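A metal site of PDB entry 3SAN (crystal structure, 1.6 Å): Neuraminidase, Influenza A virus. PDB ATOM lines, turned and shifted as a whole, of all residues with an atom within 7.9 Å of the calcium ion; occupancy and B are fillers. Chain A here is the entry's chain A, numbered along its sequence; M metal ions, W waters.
OD1 of Asp 243 lies within salt-bridge range of NH2 of Arg 220 (3.7 Å). The backbone carbonyl oxygen of Gly 269 is in hydrogen-bond range of the guanidinium group of Arg 212 (3.2 Å). N of Val 270 sits at hydrogen-bond distance from OD1 of Asp 243 (2.9 Å). OD1 of Asn 214 lies within hydrogen-bond range of N of Gly 269. The backbone carbonyl oxygen (O) of Asp 243 sits close to the guanidinium group (NH1) of Arg 246. N of Trp 215 lies within hydrogen-bond range of OD1 of Asp 213. N of Asn 216 sits at hydrogen-bond distance from OD1 of Asp 213, at 3.2 Å. The side-chain carboxylate (OD2) of Asp 213 is in hydrogen-bond range of the side-chain hydroxyl (OH) of Tyr 235, at 2.5 Å.
Gly 269 touches the calcium ion (CA to CA, 3.9 Å). Five residues have an atom within 4 Å of the calcium ion: Asp 213, Gly 217, Asp 243, Tyr 268 and Gly 269.
The calcium ion is bound by the backbone carbonyl oxygen of Asp 213 (2.4 Å), the side-chain carboxylate of Asp 243 (2.4 Å), the backbone carbonyl oxygen of Gly 217 (2.4 Å), the backbone carbonyl oxygen of Tyr 268 (2.4 Å), water W2 (2.4 Å) and water W1 (2.5 Å).
Water W2 lies within hydrogen-bond range of O of Trp 215, O of Thr 265, N of Asn 267 and N of Gly 217. Water W1 bridges the backbone carbonyl oxygen of Thr 265 (2.7 Å) and the backbone carbonyl oxygen of Pro 245 (2.7 Å).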
ATOM      1  N   HIS A 194      16.068 -23.007 -27.071  1.00  0.00           N
ATOM      2  CA  HIS A 194      16.467 -21.624 -27.284  1.00  0.00           C
ATOM      3  C   HIS A 194      17.749 -21.385 -26.532  1.00  0.00           C
ATOM      4  O   HIS A 194      17.847 -21.707 -25.344  1.00  0.00           O
ATOM      5  CB  HIS A 194      15.364 -20.685 -26.784  1.00  0.00           C
ATOM      6  CG  HIS A 194      15.431 -19.299 -27.350  1.00  0.00           C
ATOM      7  ND1 HIS A 194      15.827 -18.211 -26.604  1.00  0.00           N
ATOM      8  CD2 HIS A 194      15.141 -18.828 -28.592  1.00  0.00           C
ATOM      9  CE1 HIS A 194      15.771 -17.122 -27.364  1.00  0.00           C
ATOM     10  NE2 HIS A 194      15.370 -17.473 -28.566  1.00  0.00           N
ATOM     11  N   CYS A 211      23.561 -21.950 -20.681  1.00  0.00           N
ATOM     12  CA  CYS A 211      23.017 -20.792 -21.396  1.00  0.00           C
ATOM     13  C   CYS A 211      21.664 -20.324 -20.866  1.00  0.00           C
ATOM     14  O   CYS A 211      21.202 -20.776 -19.806  1.00  0.00           O
ATOM     15  CB  CYS A 211      22.924 -21.093 -22.895  1.00  0.00           C
ATOM     16  SG  CYS A 211      24.436 -21.885 -23.571  1.00  0.00           S
ATOM     17  N   ARG A 212      21.053 -19.404 -21.609  1.00  0.00           N
ATOM     18  CA  ARG A 212      19.741 -18.852 -21.282  1.00  0.00           C
ATOM     19  C   ARG A 212      18.741 -19.250 -22.354  1.00  0.00           C
ATOM     20  O   ARG A 212      18.997 -19.058 -23.547  1.00  0.00           O
ATOM     21  CB  ARG A 212      19.841 -17.332 -21.210  1.00  0.00           C
ATOM     22  CG  ARG A 212      18.513 -16.573 -21.232  1.00  0.00           C
ATOM     23  CD  ARG A 212      18.793 -15.061 -21.292  1.00  0.00           C
ATOM     24  NE  ARG A 212      17.590 -14.234 -21.398  1.00  0.00           N
ATOM     25  CZ  ARG A 212      17.589 -12.909 -21.250  1.00  0.00           C
ATOM     26  NH1 ARG A 212      18.713 -12.262 -20.963  1.00  0.00           N
ATOM     27  NH2 ARG A 212      16.463 -12.214 -21.359  1.00  0.00           N
ATOM     28  N   ASP A 213      17.620 -19.825 -21.938  1.00  0.00           N
ATOM     29  CA  ASP A 213      16.515 -20.113 -22.847  1.00  0.00           C
ATOM     30  C   ASP A 213      15.501 -18.998 -22.631  1.00  0.00           C
ATOM     31  O   ASP A 213      15.002 -18.831 -21.532  1.00  0.00           O
ATOM     32  CB  ASP A 213      15.927 -21.491 -22.519  1.00  0.00           C
ATOM     33  CG  ASP A 213      14.728 -21.845 -23.374  1.00  0.00           C
ATOM     34  OD1 ASP A 213      13.830 -21.004 -23.546  1.00  0.00           O
ATOM     35  OD2 ASP A 213      14.673 -22.997 -23.863  1.00  0.00           O
ATOM     36  N   ASN A 214      15.224 -18.204 -23.670  1.00  0.00           N
ATOM     37  CA  ASN A 214      14.343 -17.039 -23.515  1.00  0.00           C
ATOM     38  C   ASN A 214      12.963 -17.323 -24.088  1.00  0.00           C
ATOM     39  O   ASN A 214      12.164 -16.402 -24.332  1.00  0.00           O
ATOM     40  CB  ASN A 214      14.951 -15.817 -24.205  1.00  0.00           C
ATOM     41  CG  ASN A 214      14.518 -14.517 -23.559  1.00  0.00           C
ATOM     42  OD1 ASN A 214      14.753 -14.289 -22.366  1.00  0.00           O
ATOM     43  ND2 ASN A 214      13.907 -13.639 -24.351  1.00  0.00           N
ATOM     44  N   TRP A 215      12.680 -18.601 -24.297  1.00  0.00           N
ATOM     45  CA  TRP A 215      11.478 -19.064 -24.976  1.00  0.00           C
ATOM     46  C   TRP A 215      10.650 -19.898 -24.004  1.00  0.00           C
ATOM     47  O   TRP A 215       9.965 -19.357 -23.139  1.00  0.00           O
ATOM     48  CB  TRP A 215      11.889 -19.856 -26.219  1.00  0.00           C
ATOM     49  CG  TRP A 215      10.770 -20.298 -27.134  1.00  0.00           C
ATOM     50  CD1 TRP A 215       9.481 -19.868 -27.130  1.00  0.00           C
ATOM     51  CD2 TRP A 215      10.875 -21.248 -28.196  1.00  0.00           C
ATOM     52  NE1 TRP A 215       8.769 -20.511 -28.111  1.00  0.00           N
ATOM     53  CE2 TRP A 215       9.601 -21.358 -28.784  1.00  0.00           C
ATOM     54  CE3 TRP A 215      11.926 -22.024 -28.703  1.00  0.00           C
ATOM     55  CZ2 TRP A 215       9.343 -22.217 -29.851  1.00  0.00           C
ATOM     56  CZ3 TRP A 215      11.670 -22.868 -29.764  1.00  0.00           C
ATOM     57  CH2 TRP A 215      10.392 -22.961 -30.329  1.00  0.00           C
ATOM     58  N   ASN A 216      10.736 -21.225 -24.105  1.00  0.00           N
ATOM     59  CA  ASN A 216       9.920 -22.111 -23.279  1.00  0.00           C
ATOM     60  C   ASN A 216      10.591 -22.761 -22.070  1.00  0.00           C
ATOM     61  O   ASN A 216       9.991 -23.611 -21.418  1.00  0.00           O
ATOM     62  CB  ASN A 216       9.302 -23.214 -24.144  1.00  0.00           C
ATOM     63  CG  ASN A 216       8.257 -22.683 -25.110  1.00  0.00           C
ATOM     64  OD1 ASN A 216       8.091 -23.214 -26.218  1.00  0.00           O
ATOM     65  ND2 ASN A 216       7.546 -21.652 -24.694  1.00  0.00           N
ATOM     66  N   GLY A 217      11.825 -22.375 -21.764  1.00  0.00           N
ATOM     67  CA  GLY A 217      12.550 -23.048 -20.695  1.00  0.00           C
ATOM     68  C   GLY A 217      12.944 -22.199 -19.491  1.00  0.00           C
ATOM     69  O   GLY A 217      13.564 -21.156 -19.649  1.00  0.00           O
ATOM     70  N   MET A 218      12.589 -22.667 -18.289  1.00  0.00           N
ATOM     71  CA  MET A 218      13.072 -22.061 -17.058  1.00  0.00           C
ATOM     72  C   MET A 218      14.259 -22.885 -16.549  1.00  0.00           C
ATOM     73  O   MET A 218      14.908 -22.520 -15.568  1.00  0.00           O
ATOM     74  CB  MET A 218      11.973 -22.012 -15.998  1.00  0.00           C
ATOM     75  CG  MET A 218      11.675 -23.362 -15.359  1.00  0.00           C
ATOM     76  SD  MET A 218      10.401 -23.308 -14.076  1.00  0.00           S
ATOM     77  CE  MET A 218       8.916 -23.514 -15.049  1.00  0.00           C
ATOM     78  N   ASN A 219      14.517 -24.014 -17.217  1.00  0.00           N
ATOM     79  CA  ASN A 219      15.795 -24.699 -17.054  1.00  0.00           C
ATOM     80  C   ASN A 219      16.803 -24.188 -18.080  1.00  0.00           C
ATOM     81  O   ASN A 219      16.409 -23.613 -19.101  1.00  0.00           O
ATOM     82  CB  ASN A 219      15.648 -26.238 -17.097  1.00  0.00           C
ATOM     83  CG  ASN A 219      14.824 -26.735 -18.279  1.00  0.00           C
ATOM     84  OD1 ASN A 219      14.148 -25.973 -18.976  1.00  0.00           O
ATOM     85  ND2 ASN A 219      14.880 -28.055 -18.516  1.00  0.00           N
ATOM     86  N   ARG A 220      18.090 -24.359 -17.800  1.00  0.00           N
ATOM     87  CA  ARG A 220      19.135 -23.785 -18.650  1.00  0.00           C
ATOM     88  C   ARG A 220      19.644 -24.773 -19.684  1.00  0.00           C
ATOM     89  O   ARG A 220      19.955 -25.914 -19.344  1.00  0.00           O
ATOM     90  CB  ARG A 220      20.304 -23.286 -17.810  1.00  0.00           C
ATOM     91  CG  ARG A 220      19.967 -22.069 -16.966  1.00  0.00           C
ATOM     92  CD  ARG A 220      21.225 -21.342 -16.503  1.00  0.00           C
ATOM     93  NE  ARG A 220      20.869 -20.145 -15.738  1.00  0.00           N
ATOM     94  CZ  ARG A 220      20.488 -18.997 -16.284  1.00  0.00           C
ATOM     95  NH1 ARG A 220      20.408 -18.869 -17.603  1.00  0.00           N
ATOM     96  NH2 ARG A 220      20.172 -17.965 -15.506  1.00  0.00           N
ATOM     97  N   PRO A 221      19.745 -24.334 -20.949  1.00  0.00           N
ATOM     98  CA  PRO A 221      20.349 -25.209 -21.954  1.00  0.00           C
ATOM     99  C   PRO A 221      21.810 -25.489 -21.619  1.00  0.00           C
ATOM    100  O   PRO A 221      22.497 -24.620 -21.058  1.00  0.00           O
ATOM    101  CB  PRO A 221      20.261 -24.392 -23.243  1.00  0.00           C
ATOM    102  CG  PRO A 221      19.150 -23.429 -23.010  1.00  0.00           C
ATOM    103  CD  PRO A 221      19.217 -23.100 -21.537  1.00  0.00           C
ATOM    104  N   TYR A 235      19.471 -29.822 -21.889  1.00  0.00           N
ATOM    105  CA  TYR A 235      19.243 -28.954 -20.741  1.00  0.00           C
ATOM    106  C   TYR A 235      19.945 -29.488 -19.503  1.00  0.00           C
ATOM    107  O   TYR A 235      20.240 -30.675 -19.401  1.00  0.00           O
ATOM    108  CB  TYR A 235      17.742 -28.796 -20.481  1.00  0.00           C
ATOM    109  CG  TYR A 235      17.086 -27.880 -21.489  1.00  0.00           C
ATOM    110  CD1 TYR A 235      16.682 -28.365 -22.720  1.00  0.00           C
ATOM    111  CD2 TYR A 235      16.903 -26.533 -21.212  1.00  0.00           C
ATOM    112  CE1 TYR A 235      16.105 -27.529 -23.661  1.00  0.00           C
ATOM    113  CE2 TYR A 235      16.324 -25.689 -22.142  1.00  0.00           C
ATOM    114  CZ  TYR A 235      15.934 -26.192 -23.364  1.00  0.00           C
ATOM    115  OH  TYR A 235      15.371 -25.369 -24.311  1.00  0.00           O
ATOM    116  N   ASP A 243      16.973 -20.628 -14.056  1.00  0.00           N
ATOM    117  CA  ASP A 243      16.721 -19.404 -14.806  1.00  0.00           C
ATOM    118  C   ASP A 243      15.858 -18.487 -13.933  1.00  0.00           C
ATOM    119  O   ASP A 243      15.408 -18.885 -12.856  1.00  0.00           O
ATOM    120  CB  ASP A 243      16.005 -19.706 -16.124  1.00  0.00           C
ATOM    121  CG  ASP A 243      16.130 -18.592 -17.163  1.00  0.00           C
ATOM    122  OD1 ASP A 243      16.828 -17.574 -16.929  1.00  0.00           O
ATOM    123  OD2 ASP A 243      15.535 -18.744 -18.243  1.00  0.00           O
ATOM    124  N   THR A 244      15.643 -17.259 -14.403  1.00  0.00           N
ATOM    125  CA  THR A 244      14.686 -16.339 -13.793  1.00  0.00           C
ATOM    126  C   THR A 244      13.999 -15.634 -14.947  1.00  0.00           C
ATOM    127  O   THR A 244      14.668 -15.041 -15.780  1.00  0.00           O
ATOM    128  CB  THR A 244      15.388 -15.291 -12.905  1.00  0.00           C
ATOM    129  OG1 THR A 244      16.240 -15.952 -11.968  1.00  0.00           O
ATOM    130  CG2 THR A 244      14.360 -14.446 -12.159  1.00  0.00           C
ATOM    131  N   PRO A 245      12.658 -15.683 -14.999  1.00  0.00           N
ATOM    132  CA  PRO A 245      11.757 -16.256 -13.985  1.00  0.00           C
ATOM    133  C   PRO A 245      11.694 -17.791 -13.994  1.00  0.00           C
ATOM    134  O   PRO A 245      12.021 -18.436 -14.988  1.00  0.00           O
ATOM    135  CB  PRO A 245      10.396 -15.684 -14.367  1.00  0.00           C
ATOM    136  CG  PRO A 245      10.486 -15.497 -15.851  1.00  0.00           C
ATOM    137  CD  PRO A 245      11.905 -15.085 -16.117  1.00  0.00           C
ATOM    138  N   ARG A 246      11.242 -18.341 -12.860  1.00  0.00           N
ATOM    139  CA  ARG A 246      11.064 -19.780 -12.698  1.00  0.00           C
ATOM    140  C   ARG A 246       9.985 -20.009 -11.636  1.00  0.00           C
ATOM    141  O   ARG A 246       9.439 -19.051 -11.087  1.00  0.00           O
ATOM    142  CB  ARG A 246      12.370 -20.441 -12.254  1.00  0.00           C
ATOM    143  CG  ARG A 246      12.899 -19.922 -10.914  1.00  0.00           C
ATOM    144  CD  ARG A 246      14.217 -20.599 -10.509  1.00  0.00           C
ATOM    145  NE  ARG A 246      14.584 -20.242  -9.149  1.00  0.00           N
ATOM    146  CZ  ARG A 246      15.311 -19.171  -8.815  1.00  0.00           C
ATOM    147  NH1 ARG A 246      15.767 -18.351  -9.753  1.00  0.00           N
ATOM    148  NH2 ARG A 246      15.569 -18.921  -7.535  1.00  0.00           N
ATOM    149  N   VAL A 260      11.561 -26.968 -19.950  1.00  0.00           N
ATOM    150  CA  VAL A 260      10.491 -27.070 -18.979  1.00  0.00           C
ATOM    151  C   VAL A 260      10.108 -25.655 -18.582  1.00  0.00           C
ATOM    152  O   VAL A 260      10.927 -24.895 -18.081  1.00  0.00           O
ATOM    153  CB  VAL A 260      10.936 -27.854 -17.732  1.00  0.00           C
ATOM    154  CG1 VAL A 260       9.842 -27.863 -16.674  1.00  0.00           C
ATOM    155  CG2 VAL A 260      11.326 -29.281 -18.118  1.00  0.00           C
ATOM    156  N   GLY A 261       8.853 -25.287 -18.829  1.00  0.00           N
ATOM    157  CA  GLY A 261       8.427 -23.918 -18.631  1.00  0.00           C
ATOM    158  C   GLY A 261       6.988 -23.784 -18.180  1.00  0.00           C
ATOM    159  O   GLY A 261       6.503 -24.573 -17.360  1.00  0.00           O
ATOM    160  N   THR A 265       6.466 -18.357 -16.671  1.00  0.00           N
ATOM    161  CA  THR A 265       7.914 -18.226 -16.789  1.00  0.00           C
ATOM    162  C   THR A 265       8.408 -18.112 -18.236  1.00  0.00           C
ATOM    163  O   THR A 265       9.577 -17.845 -18.461  1.00  0.00           O
ATOM    164  CB  THR A 265       8.643 -19.427 -16.144  1.00  0.00           C
ATOM    165  OG1 THR A 265       8.461 -20.589 -16.957  1.00  0.00           O
ATOM    166  CG2 THR A 265       8.107 -19.682 -14.736  1.00  0.00           C
ATOM    167  N   ASN A 266       7.513 -18.321 -19.208  1.00  0.00           N
ATOM    168  CA  ASN A 266       7.925 -18.302 -20.613  1.00  0.00           C
ATOM    169  C   ASN A 266       8.331 -16.909 -21.099  1.00  0.00           C
ATOM    170  O   ASN A 266       7.887 -15.897 -20.548  1.00  0.00           O
ATOM    171  CB  ASN A 266       6.811 -18.837 -21.522  1.00  0.00           C
ATOM    172  CG  ASN A 266       6.557 -20.323 -21.343  1.00  0.00           C
ATOM    173  OD1 ASN A 266       5.523 -20.836 -21.778  1.00  0.00           O
ATOM    174  ND2 ASN A 266       7.493 -21.028 -20.709  1.00  0.00           N
ATOM    175  N   ASN A 267       9.170 -16.874 -22.127  1.00  0.00           N
ATOM    176  CA  ASN A 267       9.481 -15.642 -22.864  1.00  0.00           C
ATOM    177  C   ASN A 267      10.395 -14.644 -22.141  1.00  0.00           C
ATOM    178  O   ASN A 267      10.461 -13.481 -22.519  1.00  0.00           O
ATOM    179  CB  ASN A 267       8.193 -14.961 -23.345  1.00  0.00           C
ATOM    180  CG  ASN A 267       7.408 -15.848 -24.279  1.00  0.00           C
ATOM    181  OD1 ASN A 267       7.975 -16.530 -25.132  1.00  0.00           O
ATOM    182  ND2 ASN A 267       6.091 -15.851 -24.110  1.00  0.00           N
ATOM    183  N   TYR A 268      11.086 -15.103 -21.111  1.00  0.00           N
ATOM    184  CA  TYR A 268      12.132 -14.280 -20.516  1.00  0.00           C
ATOM    185  C   TYR A 268      13.177 -15.180 -19.912  1.00  0.00           C
ATOM    186  O   TYR A 268      13.126 -16.400 -20.076  1.00  0.00           O
ATOM    187  CB  TYR A 268      11.555 -13.315 -19.463  1.00  0.00           C
ATOM    188  CG  TYR A 268      12.396 -12.060 -19.254  1.00  0.00           C
ATOM    189  CD1 TYR A 268      12.848 -11.309 -20.338  1.00  0.00           C
ATOM    190  CD2 TYR A 268      12.702 -11.614 -17.973  1.00  0.00           C
ATOM    191  CE1 TYR A 268      13.597 -10.151 -20.151  1.00  0.00           C
ATOM    192  CE2 TYR A 268      13.450 -10.462 -17.773  1.00  0.00           C
ATOM    193  CZ  TYR A 268      13.898  -9.742 -18.870  1.00  0.00           C
ATOM    194  OH  TYR A 268      14.637  -8.594 -18.687  1.00  0.00           O
ATOM    195  N   GLY A 269      14.142 -14.577 -19.237  1.00  0.00           N
ATOM    196  CA  GLY A 269      15.254 -15.329 -18.691  1.00  0.00           C
ATOM    197  C   GLY A 269      16.308 -14.341 -18.240  1.00  0.00           C
ATOM    198  O   GLY A 269      16.105 -13.132 -18.293  1.00  0.00           O
ATOM    199  N   VAL A 270      17.431 -14.871 -17.781  1.00  0.00           N
ATOM    200  CA  VAL A 270      18.567 -14.050 -17.387  1.00  0.00           C
ATOM    201  C   VAL A 270      19.821 -14.853 -17.686  1.00  0.00           C
ATOM    202  O   VAL A 270      19.810 -16.077 -17.581  1.00  0.00           O
ATOM    203  CB  VAL A 270      18.493 -13.640 -15.889  1.00  0.00           C
ATOM    204  CG1 VAL A 270      18.706 -14.841 -14.959  1.00  0.00           C
ATOM    205  CG2 VAL A 270      19.519 -12.545 -15.584  1.00  0.00           C
HETATM  206 CA    CA M   1      13.604 -18.736 -19.631  1.00  0.00          CA
HETATM  207  O   HOH W   1      12.085 -18.417 -17.688  1.00  0.00           O
HETATM  208  O   HOH W   2      11.428 -19.082 -20.693  1.00  0.00           O
